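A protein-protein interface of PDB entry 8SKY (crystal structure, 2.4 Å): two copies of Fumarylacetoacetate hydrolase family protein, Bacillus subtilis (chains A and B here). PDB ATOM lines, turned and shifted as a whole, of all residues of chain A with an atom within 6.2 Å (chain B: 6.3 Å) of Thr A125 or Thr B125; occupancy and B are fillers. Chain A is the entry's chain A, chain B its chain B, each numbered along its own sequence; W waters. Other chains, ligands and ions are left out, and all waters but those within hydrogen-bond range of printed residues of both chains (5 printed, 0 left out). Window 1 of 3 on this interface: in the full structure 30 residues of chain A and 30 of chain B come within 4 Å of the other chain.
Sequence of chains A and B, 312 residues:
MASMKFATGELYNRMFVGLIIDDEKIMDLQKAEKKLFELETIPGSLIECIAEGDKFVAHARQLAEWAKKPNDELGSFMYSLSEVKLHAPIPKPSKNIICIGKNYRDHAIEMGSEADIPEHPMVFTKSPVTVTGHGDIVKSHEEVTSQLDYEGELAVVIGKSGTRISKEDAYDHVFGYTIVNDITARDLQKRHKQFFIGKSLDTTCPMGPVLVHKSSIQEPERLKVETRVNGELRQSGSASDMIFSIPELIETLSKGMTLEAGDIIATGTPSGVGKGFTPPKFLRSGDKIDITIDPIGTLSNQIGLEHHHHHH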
ATOM      1  N   ASN A  96      10.272   8.973  14.567  1.00  0.00           N
ATOM      2  CA  ASN A  96       9.671  10.042  15.286  1.00  0.00           C
ATOM      3  C   ASN A  96      10.384  11.348  15.097  1.00  0.00           C
ATOM      4  O   ASN A  96      11.566  11.393  14.874  1.00  0.00           O
ATOM      5  CB  ASN A  96       9.536   9.782  16.811  1.00  0.00           C
ATOM      6  CG  ASN A  96       8.735   8.558  17.193  1.00  0.00           C
ATOM      7  OD1 ASN A  96       8.373   8.410  18.348  1.00  0.00           O
ATOM      8  ND2 ASN A  96       8.500   7.676  16.276  1.00  0.00           N
ATOM      9  N   ILE A  97       9.630  12.413  15.161  1.00  0.00           N
ATOM     10  CA  ILE A  97      10.178  13.707  15.077  1.00  0.00           C
ATOM     11  C   ILE A  97      11.010  14.065  16.262  1.00  0.00           C
ATOM     12  O   ILE A  97      10.582  14.009  17.370  1.00  0.00           O
ATOM     13  CB  ILE A  97       9.062  14.705  14.889  1.00  0.00           C
ATOM     14  CG1 ILE A  97       8.245  14.285  13.670  1.00  0.00           C
ATOM     15  CG2 ILE A  97       9.611  16.113  14.742  1.00  0.00           C
ATOM     16  CD1 ILE A  97       7.156  15.241  13.296  1.00  0.00           C
ATOM     17  N   ILE A  98      12.227  14.435  15.974  1.00  0.00           N
ATOM     18  CA  ILE A  98      13.162  14.808  17.028  1.00  0.00           C
ATOM     19  C   ILE A  98      12.897  16.256  17.415  1.00  0.00           C
ATOM     20  O   ILE A  98      12.852  17.142  16.554  1.00  0.00           O
ATOM     21  CB  ILE A  98      14.610  14.605  16.558  1.00  0.00           C
ATOM     22  CG1 ILE A  98      14.827  13.149  16.137  1.00  0.00           C
ATOM     23  CG2 ILE A  98      15.581  14.991  17.654  1.00  0.00           C
ATOM     24  CD1 ILE A  98      16.228  12.848  15.643  1.00  0.00           C
ATOM     25  N   CYS A  99      12.703  16.503  18.708  1.00  0.00           N
ATOM     26  CA  CYS A  99      12.310  17.821  19.183  1.00  0.00           C
ATOM     27  C   CYS A  99      13.264  18.314  20.259  1.00  0.00           C
ATOM     28  O   CYS A  99      13.739  17.535  21.091  1.00  0.00           O
ATOM     29  CB  CYS A  99      10.880  17.814  19.732  1.00  0.00           C
ATOM     30  SG  CYS A  99       9.611  17.259  18.571  1.00  0.00           S
ATOM     31  N   VAL A 123      16.203  16.852  24.557  1.00  0.00           N
ATOM     32  CA  VAL A 123      15.710  16.280  23.312  1.00  0.00           C
ATOM     33  C   VAL A 123      14.703  15.180  23.617  1.00  0.00           C
ATOM     34  O   VAL A 123      14.964  14.296  24.439  1.00  0.00           O
ATOM     35  CB  VAL A 123      16.865  15.743  22.446  1.00  0.00           C
ATOM     36  CG1 VAL A 123      16.347  15.285  21.105  1.00  0.00           C
ATOM     37  CG2 VAL A 123      17.915  16.825  22.252  1.00  0.00           C
ATOM     38  N   PHE A 124      13.557  15.240  22.940  1.00  0.00           N
ATOM     39  CA  PHE A 124      12.477  14.270  23.060  1.00  0.00           C
ATOM     40  C   PHE A 124      11.905  14.059  21.661  1.00  0.00           C
ATOM     41  O   PHE A 124      12.426  14.591  20.676  1.00  0.00           O
ATOM     42  CB  PHE A 124      11.436  14.765  24.071  1.00  0.00           C
ATOM     43  CG  PHE A 124      10.825  16.083  23.703  1.00  0.00           C
ATOM     44  CD1 PHE A 124       9.687  16.141  22.919  1.00  0.00           C
ATOM     45  CD2 PHE A 124      11.412  17.270  24.113  1.00  0.00           C
ATOM     46  CE1 PHE A 124       9.133  17.353  22.572  1.00  0.00           C
ATOM     47  CE2 PHE A 124      10.863  18.486  23.767  1.00  0.00           C
ATOM     48  CZ  PHE A 124       9.722  18.528  22.994  1.00  0.00           C
ATOM     49  N   THR A 125      10.820  13.289  21.555  1.00  0.00           N
ATOM     50  CA  THR A 125      10.280  12.944  20.246  1.00  0.00           C
ATOM     51  C   THR A 125       8.761  13.056  20.222  1.00  0.00           C
ATOM     52  O   THR A 125       8.090  13.010  21.257  1.00  0.00           O
ATOM     53  CB  THR A 125      10.681  11.526  19.810  1.00  0.00           C
ATOM     54  OG1 THR A 125      10.174  10.569  20.748  1.00  0.00           O
ATOM     55  CG2 THR A 125      12.192  11.395  19.705  1.00  0.00           C
ATOM     56  N   LYS A 126       8.234  13.211  19.006  1.00  0.00           N
ATOM     57  CA  LYS A 126       6.806  13.133  18.715  1.00  0.00           C
ATOM     58  C   LYS A 126       6.556  11.972  17.767  1.00  0.00           C
ATOM     59  O   LYS A 126       7.208  11.873  16.723  1.00  0.00           O
ATOM     60  CB  LYS A 126       6.286  14.420  18.072  1.00  0.00           C
ATOM     61  CG  LYS A 126       6.328  15.645  18.947  1.00  0.00           C
ATOM     62  CD  LYS A 126       5.827  16.849  18.172  1.00  0.00           C
ATOM     63  CE  LYS A 126       4.308  16.856  18.108  1.00  0.00           C
ATOM     64  NZ  LYS A 126       3.701  17.553  19.274  1.00  0.00           N
ATOM     65  N   SER A 127       5.579  11.132  18.102  1.00  0.00           N
ATOM     66  CA  SER A 127       5.267   9.972  17.282  1.00  0.00           C
ATOM     67  C   SER A 127       4.807  10.407  15.889  1.00  0.00           C
ATOM     68  O   SER A 127       4.227  11.485  15.727  1.00  0.00           O
ATOM     69  CB  SER A 127       4.181   9.130  17.950  1.00  0.00           C
ATOM     70  OG  SER A 127       3.726   8.091  17.100  1.00  0.00           O
ATOM     71  N   PHE A 195       8.425  13.659  28.199  1.00  0.00           N
ATOM     72  CA  PHE A 195       7.523  14.485  27.418  1.00  0.00           C
ATOM     73  C   PHE A 195       6.701  13.688  26.412  1.00  0.00           C
ATOM     74  O   PHE A 195       5.752  14.243  25.851  1.00  0.00           O
ATOM     75  CB  PHE A 195       8.322  15.573  26.705  1.00  0.00           C
ATOM     76  CG  PHE A 195       8.854  16.630  27.629  1.00  0.00           C
ATOM     77  CD1 PHE A 195       8.405  16.711  28.938  1.00  0.00           C
ATOM     78  CD2 PHE A 195       9.810  17.531  27.201  1.00  0.00           C
ATOM     79  CE1 PHE A 195       8.892  17.676  29.797  1.00  0.00           C
ATOM     80  CE2 PHE A 195      10.301  18.498  28.056  1.00  0.00           C
ATOM     81  CZ  PHE A 195       9.842  18.570  29.356  1.00  0.00           C
ATOM     82  N   PHE A 196       7.005  12.402  26.213  1.00  0.00           N
ATOM     83  CA  PHE A 196       6.543  11.696  25.021  1.00  0.00           C
ATOM     84  C   PHE A 196       5.021  11.677  24.910  1.00  0.00           C
ATOM     85  O   PHE A 196       4.464  12.033  23.866  1.00  0.00           O
ATOM     86  CB  PHE A 196       7.090  10.270  25.009  1.00  0.00           C
ATOM     87  CG  PHE A 196       6.494   9.411  23.936  1.00  0.00           C
ATOM     88  CD1 PHE A 196       6.770   9.667  22.603  1.00  0.00           C
ATOM     89  CD2 PHE A 196       5.649   8.363  24.253  1.00  0.00           C
ATOM     90  CE1 PHE A 196       6.220   8.888  21.605  1.00  0.00           C
ATOM     91  CE2 PHE A 196       5.097   7.578  23.258  1.00  0.00           C
ATOM     92  CZ  PHE A 196       5.383   7.843  21.932  1.00  0.00           C
ATOM     93  N   LYS A 199       3.299  14.849  24.166  1.00  0.00           N
ATOM     94  CA  LYS A 199       3.749  15.365  22.883  1.00  0.00           C
ATOM     95  C   LYS A 199       3.270  14.532  21.701  1.00  0.00           C
ATOM     96  O   LYS A 199       3.519  14.914  20.554  1.00  0.00           O
ATOM     97  CB  LYS A 199       5.280  15.437  22.854  1.00  0.00           C
ATOM     98  CG  LYS A 199       5.882  16.503  23.747  1.00  0.00           C
ATOM     99  CD  LYS A 199       5.744  17.881  23.138  1.00  0.00           C
ATOM    100  CE  LYS A 199       6.438  18.922  23.999  1.00  0.00           C
ATOM    101  NZ  LYS A 199       6.409  20.267  23.366  1.00  0.00           N
ATOM    102  N   SER A 200       2.591  13.409  21.945  1.00  0.00           N
ATOM    103  CA  SER A 200       2.328  12.435  20.892  1.00  0.00           C
ATOM    104  C   SER A 200       0.844  12.120  20.722  1.00  0.00           C
ATOM    105  O   SER A 200       0.501  11.071  20.169  1.00  0.00           O
ATOM    106  CB  SER A 200       3.114  11.150  21.150  1.00  0.00           C
ATOM    107  OG  SER A 200       4.508  11.404  21.123  1.00  0.00           O
ATOM    108  N   ASN B  96       9.519   4.819  16.598  1.00  0.00           N
ATOM    109  CA  ASN B  96      10.405   4.546  17.706  1.00  0.00           C
ATOM    110  C   ASN B  96       9.812   3.558  18.677  1.00  0.00           C
ATOM    111  O   ASN B  96       8.621   3.543  18.891  1.00  0.00           O
ATOM    112  CB  ASN B  96      10.840   5.814  18.460  1.00  0.00           C
ATOM    113  CG  ASN B  96      11.564   6.822  17.608  1.00  0.00           C
ATOM    114  OD1 ASN B  96      11.442   6.839  16.405  1.00  0.00           O
ATOM    115  ND2 ASN B  96      12.278   7.713  18.253  1.00  0.00           N
ATOM    116  N   ILE B  97      10.659   2.734  19.256  1.00  0.00           N
ATOM    117  CA  ILE B  97      10.220   1.775  20.219  1.00  0.00           C
ATOM    118  C   ILE B  97       9.733   2.429  21.465  1.00  0.00           C
ATOM    119  O   ILE B  97      10.398   3.239  22.030  1.00  0.00           O
ATOM    120  CB  ILE B  97      11.292   0.719  20.525  1.00  0.00           C
ATOM    121  CG1 ILE B  97      11.576  -0.084  19.265  1.00  0.00           C
ATOM    122  CG2 ILE B  97      10.874  -0.192  21.663  1.00  0.00           C
ATOM    123  CD1 ILE B  97      12.916  -0.758  19.281  1.00  0.00           C
ATOM    124  N   ILE B  98       8.551   2.045  21.884  1.00  0.00           N
ATOM    125  CA  ILE B  98       7.947   2.670  23.056  1.00  0.00           C
ATOM    126  C   ILE B  98       8.427   1.936  24.304  1.00  0.00           C
ATOM    127  O   ILE B  98       8.250   0.719  24.424  1.00  0.00           O
ATOM    128  CB  ILE B  98       6.414   2.654  22.962  1.00  0.00           C
ATOM    129  CG1 ILE B  98       5.956   3.260  21.633  1.00  0.00           C
ATOM    130  CG2 ILE B  98       5.801   3.404  24.130  1.00  0.00           C
ATOM    131  CD1 ILE B  98       4.459   3.484  21.541  1.00  0.00           C
ATOM    132  N   CYS B  99       9.024   2.673  25.239  1.00  0.00           N
ATOM    133  CA  CYS B  99       9.622   2.086  26.430  1.00  0.00           C
ATOM    134  C   CYS B  99       8.949   2.612  27.689  1.00  0.00           C
ATOM    135  O   CYS B  99       8.609   3.796  27.780  1.00  0.00           O
ATOM    136  CB  CYS B  99      11.125   2.368  26.490  1.00  0.00           C
ATOM    137  SG  CYS B  99      12.070   1.712  25.099  1.00  0.00           S
ATOM    138  N   VAL B 123       6.864   7.077  30.176  1.00  0.00           N
ATOM    139  CA  VAL B 123       7.004   6.525  28.834  1.00  0.00           C
ATOM    140  C   VAL B 123       7.951   7.390  28.014  1.00  0.00           C
ATOM    141  O   VAL B 123       7.830   8.620  28.003  1.00  0.00           O
ATOM    142  CB  VAL B 123       5.641   6.403  28.128  1.00  0.00           C
ATOM    143  CG1 VAL B 123       5.817   5.787  26.760  1.00  0.00           C
ATOM    144  CG2 VAL B 123       4.684   5.567  28.970  1.00  0.00           C
ATOM    145  N   PHE B 124       8.882   6.737  27.322  1.00  0.00           N
ATOM    146  CA  PHE B 124       9.832   7.366  26.414  1.00  0.00           C
ATOM    147  C   PHE B 124      10.045   6.410  25.243  1.00  0.00           C
ATOM    148  O   PHE B 124       9.328   5.415  25.098  1.00  0.00           O
ATOM    149  CB  PHE B 124      11.140   7.691  27.142  1.00  0.00           C
ATOM    150  CG  PHE B 124      11.836   6.478  27.662  1.00  0.00           C
ATOM    151  CD1 PHE B 124      11.431   5.883  28.845  1.00  0.00           C
ATOM    152  CD2 PHE B 124      12.865   5.901  26.944  1.00  0.00           C
ATOM    153  CE1 PHE B 124      12.060   4.756  29.316  1.00  0.00           C
ATOM    154  CE2 PHE B 124      13.491   4.773  27.408  1.00  0.00           C
ATOM    155  CZ  PHE B 124      13.095   4.199  28.598  1.00  0.00           C
ATOM    156  N   THR B 125      11.042   6.693  24.401  1.00  0.00           N
ATOM    157  CA  THR B 125      11.220   5.941  23.161  1.00  0.00           C
ATOM    158  C   THR B 125      12.696   5.740  22.830  1.00  0.00           C
ATOM    159  O   THR B 125      13.575   6.433  23.350  1.00  0.00           O
ATOM    160  CB  THR B 125      10.539   6.634  21.971  1.00  0.00           C
ATOM    161  OG1 THR B 125      11.188   7.883  21.704  1.00  0.00           O
ATOM    162  CG2 THR B 125       9.067   6.883  22.245  1.00  0.00           C
ATOM    163  N   LYS B 126      12.950   4.772  21.943  1.00  0.00           N
ATOM    164  CA  LYS B 126      14.260   4.528  21.343  1.00  0.00           C
ATOM    165  C   LYS B 126      14.148   4.625  19.826  1.00  0.00           C
ATOM    166  O   LYS B 126      13.253   4.014  19.232  1.00  0.00           O
ATOM    167  CB  LYS B 126      14.809   3.148  21.718  1.00  0.00           C
ATOM    168  CG  LYS B 126      15.123   2.940  23.187  1.00  0.00           C
ATOM    169  CD  LYS B 126      15.500   1.488  23.448  1.00  0.00           C
ATOM    170  CE  LYS B 126      16.973   1.233  23.161  1.00  0.00           C
ATOM    171  NZ  LYS B 126      17.850   1.651  24.290  1.00  0.00           N
ATOM    172  N   SER B 127      15.078   5.353  19.200  1.00  0.00           N
ATOM    173  CA  SER B 127      15.042   5.566  17.755  1.00  0.00           C
ATOM    174  C   SER B 127      15.171   4.240  17.006  1.00  0.00           C
ATOM    175  O   SER B 127      15.832   3.324  17.481  1.00  0.00           O
ATOM    176  CB  SER B 127      16.159   6.513  17.321  1.00  0.00           C
ATOM    177  OG  SER B 127      16.270   6.551  15.910  1.00  0.00           O
ATOM    178  N   PHE B 195      15.117  11.095  28.232  1.00  0.00           N
ATOM    179  CA  PHE B 195      15.868   9.861  28.078  1.00  0.00           C
ATOM    180  C   PHE B 195      16.300   9.594  26.645  1.00  0.00           C
ATOM    181  O   PHE B 195      17.103   8.679  26.431  1.00  0.00           O
ATOM    182  CB  PHE B 195      15.041   8.689  28.597  1.00  0.00           C
ATOM    183  CG  PHE B 195      14.988   8.602  30.093  1.00  0.00           C
ATOM    184  CD1 PHE B 195      15.506   9.615  30.889  1.00  0.00           C
ATOM    185  CD2 PHE B 195      14.429   7.499  30.705  1.00  0.00           C
ATOM    186  CE1 PHE B 195      15.457   9.525  32.267  1.00  0.00           C
ATOM    187  CE2 PHE B 195      14.382   7.402  32.075  1.00  0.00           C
ATOM    188  CZ  PHE B 195      14.894   8.417  32.859  1.00  0.00           C
ATOM    189  N   PHE B 196      15.822  10.376  25.676  1.00  0.00           N
ATOM    190  CA  PHE B 196      15.898   9.949  24.281  1.00  0.00           C
ATOM    191  C   PHE B 196      17.338   9.746  23.823  1.00  0.00           C
ATOM    192  O   PHE B 196      17.668   8.709  23.239  1.00  0.00           O
ATOM    193  CB  PHE B 196      15.192  10.950  23.372  1.00  0.00           C
ATOM    194  CG  PHE B 196      15.411  10.676  21.915  1.00  0.00           C
ATOM    195  CD1 PHE B 196      14.822   9.577  21.315  1.00  0.00           C
ATOM    196  CD2 PHE B 196      16.224  11.499  21.151  1.00  0.00           C
ATOM    197  CE1 PHE B 196      15.026   9.306  19.979  1.00  0.00           C
ATOM    198  CE2 PHE B 196      16.432  11.233  19.809  1.00  0.00           C
ATOM    199  CZ  PHE B 196      15.831  10.136  19.223  1.00  0.00           C
ATOM    200  N   LYS B 199      19.131   6.801  25.328  1.00  0.00           N
ATOM    201  CA  LYS B 199      18.506   5.538  24.968  1.00  0.00           C
ATOM    202  C   LYS B 199      18.610   5.207  23.485  1.00  0.00           C
ATOM    203  O   LYS B 199      18.199   4.116  23.084  1.00  0.00           O
ATOM    204  CB  LYS B 199      17.031   5.553  25.380  1.00  0.00           C
ATOM    205  CG  LYS B 199      16.799   5.583  26.879  1.00  0.00           C
ATOM    206  CD  LYS B 199      16.830   4.187  27.473  1.00  0.00           C
ATOM    207  CE  LYS B 199      16.505   4.227  28.959  1.00  0.00           C
ATOM    208  NZ  LYS B 199      16.625   2.889  29.599  1.00  0.00           N
ATOM    209  N   SER B 200      19.149   6.101  22.658  1.00  0.00           N
ATOM    210  CA  SER B 200      19.018   5.948  21.212  1.00  0.00           C
ATOM    211  C   SER B 200      20.369   5.972  20.510  1.00  0.00           C
ATOM    212  O   SER B 200      20.498   6.498  19.401  1.00  0.00           O
ATOM    213  CB  SER B 200      18.102   7.026  20.637  1.00  0.00           C
ATOM    214  OG  SER B 200      16.792   6.927  21.172  1.00  0.00           O
HETATM  215  O   HOH W   1      11.162  10.420  23.586  1.00  0.00           O
HETATM  216  O   HOH W   2      13.152   9.576  16.525  1.00  0.00           O
HETATM  217  O   HOH W   3      17.291  13.077  25.152  1.00  0.00           O
HETATM  218  O   HOH W   4       7.224   6.056  18.843  1.00  0.00           O
HETATM  219  O   HOH W   5       5.923  10.284  28.304  1.00  0.00           O
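ND2 of Asn A96 sits close to N of Asn B96 (3.1 Å). OG1 of Thr B125 lies within hydrogen-bond range of OG1 of Thr A125, at 3.0 Å.
Water W5 bridges O of Val B123 and N of Phe A196. Water W4 lies within hydrogen-bond range of OD1 of Asn A96 (2.7 Å) and O of Asn B96 (2.9 Å). Water W2 bridges ND2 of Asn B96 (2.7 Å) and O of Asn A96 (2.9 Å). Water W3 bridges O of Val A123 (2.7 Å) and N of Phe B196 (3.1 Å). Water W1 bridges the side-chain hydroxyl of Thr A125 (3.0 Å) and the side-chain hydroxyl of Thr B125 (3.2 Å).
Hydrophobic or aromatic side chains of chain B that line the printed part of chain A: Val B123 and Phe B196. Along chain B the printed residues that touch a printed residue of chain A span positions 96 to 196. Among the printed residues, 7 pairs touch across the chains.
The side-chain hydroxyl of Ser A200 lies within hydrogen-bond range of the backbone carbonyl oxygen of Phe A196, at 2.8 Å. The backbone carbonyl oxygen (O) of Phe B196 is in hydrogen-bond range of the side-chain hydroxyl (OG) of Ser B200, 2.9 Å away.
Printed residues of chain B within 4 Å of Asn A96: Asn B96. Printed residues of chain B within 4 Å of Thr A125: Asn B96 (3.96 Å), Thr B125 (3.0 Å) and Phe B196 (3.5 Å). Of the printed residues of chain B, Phe A196 touches Val B123 (3.5 Å) and Thr B125 (3.5 Å). Ser B200 touches none of the printed residues of chain A. The nearest residue of chain B that does not touch Thr A125 is Phe B124 (6.1 Å). The nearest printed residue of chain B that does not touch Phe A196 is Phe B124 (4.2 Å).
Among the printed residues, pairs that only touch across the chains: Phe A196 with Val B123 (3.5 Å), Val A123 with Phe B196 (3.5 Å), Thr A125 with Phe B196 (3.5 Å), Phe A196 with Thr B125 (3.5 Å) and Thr A125 with Asn B96 (3.96 Å).
Asn A96 touches its own counterpart, Asn B96. Thr A125 touches Asn B96, but with the chains exchanged Asn A96 does not touch Thr B125 (4.2 Å). Thr B125 touches its own counterpart, Thr A125. Thr A125 touches Phe B196, and with the chains exchanged Phe A196 touches Thr B125. Positions printed for both chains: 96, 97, 98, 99, 123, 124, 125, 126, 127, 195, 196, 199 and 200. Of the 7 pairs that touch across the chains among the printed residues, 6 have their exchanged pair printed and touching as well.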
